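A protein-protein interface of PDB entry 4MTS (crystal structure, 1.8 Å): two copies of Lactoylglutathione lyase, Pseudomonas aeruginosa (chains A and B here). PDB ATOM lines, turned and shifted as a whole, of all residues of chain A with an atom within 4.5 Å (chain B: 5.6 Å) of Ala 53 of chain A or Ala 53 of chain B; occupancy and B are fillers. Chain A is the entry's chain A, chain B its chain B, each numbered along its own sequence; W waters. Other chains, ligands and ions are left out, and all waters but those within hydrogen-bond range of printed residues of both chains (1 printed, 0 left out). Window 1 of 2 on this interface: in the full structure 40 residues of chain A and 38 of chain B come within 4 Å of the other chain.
O of Leu 4 of chain A lies within hydrogen-bond range of N of Ala 54 of chain A (3.0 Å). N of Ala 54 of chain B is in hydrogen-bond range of O of Leu 4 of chain B, 3.0 Å away.
Among the printed residues, pairs that only touch across the chains: Ile 3 of chain A with Ala 53 of chain B (3.5 Å), Ile 3 of chain A with Ala 54 of chain B (3.8 Å), Ile 3 of chain A with Leu 55 of chain B (3.9 Å), Ala 53 of chain A with Ile 3 of chain B (3.4 Å), Ala 53 of chain A with Ala 53 of chain B (3.9 Å) and Ala 54 of chain A with Ile 3 of chain B (3.96 Å).
Of chain B, only Ile 3 (3.4 Å) and Ala 53 (3.9 Å) come within 4 Å of Ala 53 of chain A. Of chain A, only Ile 3 and Ala 53 come within 4 Å of Ala 53 of chain B. Of the printed residues of chain A, Ala 54 of chain B touches Ile 3. Of the printed residues of chain B, Ala 54 of chain A touches Ile 3. Of the printed residues of chain B, Ile 3 of chain A touches Ala 53, Ala 54 and Leu 55. Printed residues of chain A within 4 Å of Ile 3 of chain B: Ala 53 (3.4 Å) and Ala 54 (3.96 Å). Printed residues of chain A within 4 Å of Leu 55 of chain B: Ile 3. His 5 of chain B touches none of the printed residues of chain A. Gly 45 of chain B touches none of the printed residues of chain A. The nearest printed residue of chain A that does not touch Ile 3 of chain B is Ala 52 of chain A (6.7 Å).
Hydrophobic or aromatic side chains of chain B that line the printed part of chain A: Ile 3 and Ala 53. Among the printed residues, no Asp or Glu carboxylate lies within 4 Å of a Lys or Arg side-chain nitrogen of the other chain.
Ile 3 of chain A touches Ala 53 of chain B, and with the chains exchanged Ala 53 of chain A touches Ile 3 of chain B. Ile 3 of chain A touches Ala 54 of chain B, and with the chains exchanged Ala 54 of chain A touches Ile 3 of chain B. Ala 53 of chain A touches its own counterpart, Ala 53 of chain B. 5 positions are printed for both chains. Of the 6 pairs that touch across the chains among the printed residues, 5 have their exchanged pair printed and touching as well.
Water W1 lies within hydrogen-bond range of N of Ala 53 of chain B (3.0 Å) and N of Ala 53 of chain A (3.1 Å).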
ATOM      1  N   ILE A   3     -19.434 -28.970 -22.017  1.00  0.00           N
ATOM      2  CA  ILE A   3     -17.972 -29.072 -21.915  1.00  0.00           C
ATOM      3  C   ILE A   3     -17.501 -27.813 -21.185  1.00  0.00           C
ATOM      4  O   ILE A   3     -17.834 -26.696 -21.581  1.00  0.00           O
ATOM      5  CB  ILE A   3     -17.323 -29.204 -23.327  1.00  0.00           C
ATOM      6  CG1 ILE A   3     -17.740 -30.554 -23.950  1.00  0.00           C
ATOM      7  CG2 ILE A   3     -15.784 -29.105 -23.225  1.00  0.00           C
ATOM      8  CD1 ILE A   3     -17.311 -30.770 -25.438  1.00  0.00           C
ATOM      9  N   LEU A   4     -16.700 -27.987 -20.133  1.00  0.00           N
ATOM     10  CA  LEU A   4     -16.244 -26.856 -19.316  1.00  0.00           C
ATOM     11  C   LEU A   4     -14.847 -26.365 -19.714  1.00  0.00           C
ATOM     12  O   LEU A   4     -14.644 -25.153 -19.806  1.00  0.00           O
ATOM     13  CB  LEU A   4     -16.238 -27.219 -17.833  1.00  0.00           C
ATOM     14  CG  LEU A   4     -17.611 -27.497 -17.203  1.00  0.00           C
ATOM     15  CD1 LEU A   4     -17.433 -28.032 -15.827  1.00  0.00           C
ATOM     16  CD2 LEU A   4     -18.431 -26.243 -17.125  1.00  0.00           C
ATOM     17  N   ALA A  52     -19.066 -20.560 -21.679  1.00  0.00           N
ATOM     18  CA  ALA A  52     -18.393 -21.329 -22.712  1.00  0.00           C
ATOM     19  C   ALA A  52     -17.226 -22.092 -22.165  1.00  0.00           C
ATOM     20  O   ALA A  52     -16.709 -21.764 -21.082  1.00  0.00           O
ATOM     21  CB  ALA A  52     -17.893 -20.378 -23.803  1.00  0.00           C
ATOM     22  N   ALA A  53     -16.765 -23.066 -22.967  1.00  0.00           N
ATOM     23  CA  ALA A  53     -15.577 -23.853 -22.621  1.00  0.00           C
ATOM     24  C   ALA A  53     -14.349 -22.962 -22.673  1.00  0.00           C
ATOM     25  O   ALA A  53     -14.226 -22.073 -23.530  1.00  0.00           O
ATOM     26  CB  ALA A  53     -15.405 -25.016 -23.584  1.00  0.00           C
ATOM     27  N   ALA A  54     -13.437 -23.185 -21.720  1.00  0.00           N
ATOM     28  CA  ALA A  54     -12.199 -22.428 -21.599  1.00  0.00           C
ATOM     29  C   ALA A  54     -11.013 -23.371 -21.695  1.00  0.00           C
ATOM     30  O   ALA A  54     -11.177 -24.606 -21.749  1.00  0.00           O
ATOM     31  CB  ALA A  54     -12.185 -21.722 -20.255  1.00  0.00           C
ATOM     32  N   ARG B   2     -13.701 -17.611 -31.063  1.00  0.00           N
ATOM     33  CA  ARG B   2     -14.221 -18.558 -30.066  1.00  0.00           C
ATOM     34  C   ARG B   2     -13.447 -19.851 -30.129  1.00  0.00           C
ATOM     35  O   ARG B   2     -12.877 -20.155 -31.162  1.00  0.00           O
ATOM     36  CB  ARG B   2     -15.749 -18.807 -30.179  1.00  0.00           C
ATOM     37  CG  ARG B   2     -16.181 -19.549 -31.416  1.00  0.00           C
ATOM     38  CD  ARG B   2     -17.693 -19.618 -31.552  1.00  0.00           C
ATOM     39  NE  ARG B   2     -17.988 -20.309 -32.799  1.00  0.00           N
ATOM     40  CZ  ARG B   2     -18.433 -21.553 -32.904  1.00  0.00           C
ATOM     41  NH1 ARG B   2     -18.673 -22.279 -31.813  1.00  0.00           N
ATOM     42  NH2 ARG B   2     -18.659 -22.080 -34.095  1.00  0.00           N
ATOM     43  N   ILE B   3     -13.465 -20.632 -29.056  1.00  0.00           N
ATOM     44  CA  ILE B   3     -12.846 -21.976 -29.079  1.00  0.00           C
ATOM     45  C   ILE B   3     -13.819 -22.890 -29.810  1.00  0.00           C
ATOM     46  O   ILE B   3     -15.016 -22.929 -29.481  1.00  0.00           O
ATOM     47  CB  ILE B   3     -12.558 -22.472 -27.636  1.00  0.00           C
ATOM     48  CG1 ILE B   3     -11.498 -21.582 -26.988  1.00  0.00           C
ATOM     49  CG2 ILE B   3     -12.146 -23.971 -27.631  1.00  0.00           C
ATOM     50  CD1 ILE B   3     -11.400 -21.764 -25.425  1.00  0.00           C
ATOM     51  N   LEU B   4     -13.313 -23.644 -30.793  1.00  0.00           N
ATOM     52  CA  LEU B   4     -14.165 -24.530 -31.580  1.00  0.00           C
ATOM     53  C   LEU B   4     -14.188 -25.956 -31.075  1.00  0.00           C
ATOM     54  O   LEU B   4     -15.247 -26.582 -31.088  1.00  0.00           O
ATOM     55  CB  LEU B   4     -13.739 -24.524 -33.045  1.00  0.00           C
ATOM     56  CG  LEU B   4     -13.996 -23.232 -33.816  1.00  0.00           C
ATOM     57  CD1 LEU B   4     -13.231 -23.247 -35.105  1.00  0.00           C
ATOM     58  CD2 LEU B   4     -15.491 -23.035 -34.029  1.00  0.00           C
ATOM     59  N   HIS B   5     -12.998 -26.515 -30.769  1.00  0.00           N
ATOM     60  CA  HIS B   5     -12.902 -27.872 -30.277  1.00  0.00           C
ATOM     61  C   HIS B   5     -11.531 -28.191 -29.696  1.00  0.00           C
ATOM     62  O   HIS B   5     -10.566 -27.477 -29.914  1.00  0.00           O
ATOM     63  CB  HIS B   5     -13.200 -28.892 -31.425  1.00  0.00           C
ATOM     64  CG  HIS B   5     -12.339 -28.781 -32.650  1.00  0.00           C
ATOM     65  ND1 HIS B   5     -12.817 -28.184 -33.804  1.00  0.00           N
ATOM     66  CD2 HIS B   5     -11.127 -29.328 -32.912  1.00  0.00           C
ATOM     67  CE1 HIS B   5     -11.853 -28.324 -34.710  1.00  0.00           C
ATOM     68  NE2 HIS B   5     -10.831 -29.032 -34.239  1.00  0.00           N
ATOM     69  N   GLY B  45     -20.489 -33.837 -28.706  1.00  0.00           N
ATOM     70  CA  GLY B  45     -20.708 -32.715 -27.802  1.00  0.00           C
ATOM     71  C   GLY B  45     -22.133 -32.692 -27.299  1.00  0.00           C
ATOM     72  O   GLY B  45     -22.856 -33.679 -27.451  1.00  0.00           O
ATOM     73  N   GLU B  49     -22.387 -27.391 -32.890  1.00  0.00           N
ATOM     74  CA  GLU B  49     -21.033 -26.854 -33.089  1.00  0.00           C
ATOM     75  C   GLU B  49     -20.980 -25.345 -33.306  1.00  0.00           C
ATOM     76  O   GLU B  49     -19.971 -24.724 -32.957  1.00  0.00           O
ATOM     77  CB  GLU B  49     -20.325 -27.549 -34.250  1.00  0.00           C
ATOM     78  CG  GLU B  49     -19.828 -28.935 -33.870  1.00  0.00           C
ATOM     79  CD  GLU B  49     -19.106 -29.612 -35.009  1.00  0.00           C
ATOM     80  OE1 GLU B  49     -17.857 -29.546 -35.027  1.00  0.00           O
ATOM     81  OE2 GLU B  49     -19.786 -30.179 -35.898  1.00  0.00           O
ATOM     82  N   ALA B  51     -22.684 -23.158 -31.797  1.00  0.00           N
ATOM     83  CA  ALA B  51     -22.970 -22.534 -30.500  1.00  0.00           C
ATOM     84  C   ALA B  51     -21.933 -22.808 -29.434  1.00  0.00           C
ATOM     85  O   ALA B  51     -21.879 -22.064 -28.452  1.00  0.00           O
ATOM     86  CB  ALA B  51     -24.308 -23.043 -29.985  1.00  0.00           C
ATOM     87  N   ALA B  52     -21.176 -23.934 -29.548  1.00  0.00           N
ATOM     88  CA  ALA B  52     -20.281 -24.283 -28.434  1.00  0.00           C
ATOM     89  C   ALA B  52     -19.143 -25.155 -28.893  1.00  0.00           C
ATOM     90  O   ALA B  52     -19.254 -25.819 -29.927  1.00  0.00           O
ATOM     91  CB  ALA B  52     -21.084 -25.033 -27.366  1.00  0.00           C
ATOM     92  N   ALA B  53     -18.084 -25.240 -28.047  1.00  0.00           N
ATOM     93  CA  ALA B  53     -16.935 -26.053 -28.350  1.00  0.00           C
ATOM     94  C   ALA B  53     -17.317 -27.533 -28.239  1.00  0.00           C
ATOM     95  O   ALA B  53     -18.057 -27.936 -27.330  1.00  0.00           O
ATOM     96  CB  ALA B  53     -15.785 -25.715 -27.400  1.00  0.00           C
ATOM     97  N   ALA B  54     -16.759 -28.338 -29.128  1.00  0.00           N
ATOM     98  CA  ALA B  54     -17.008 -29.770 -29.145  1.00  0.00           C
ATOM     99  C   ALA B  54     -15.707 -30.543 -28.899  1.00  0.00           C
ATOM    100  O   ALA B  54     -14.644 -29.946 -28.698  1.00  0.00           O
ATOM    101  CB  ALA B  54     -17.573 -30.145 -30.509  1.00  0.00           C
ATOM    102  N   LEU B  55     -15.792 -31.870 -28.910  1.00  0.00           N
ATOM    103  CA  LEU B  55     -14.622 -32.730 -28.814  1.00  0.00           C
ATOM    104  C   LEU B  55     -14.474 -33.421 -30.173  1.00  0.00           C
ATOM    105  O   LEU B  55     -15.378 -34.147 -30.613  1.00  0.00           O
ATOM    106  CB  LEU B  55     -14.784 -33.773 -27.687  1.00  0.00           C
ATOM    107  CG  LEU B  55     -13.743 -34.907 -27.642  1.00  0.00           C
ATOM    108  CD1 LEU B  55     -12.264 -34.346 -27.367  1.00  0.00           C
ATOM    109  CD2 LEU B  55     -14.141 -35.940 -26.622  1.00  0.00           C
HETATM  110  O   HOH W   1     -18.250 -23.529 -25.629  1.00  0.00           O
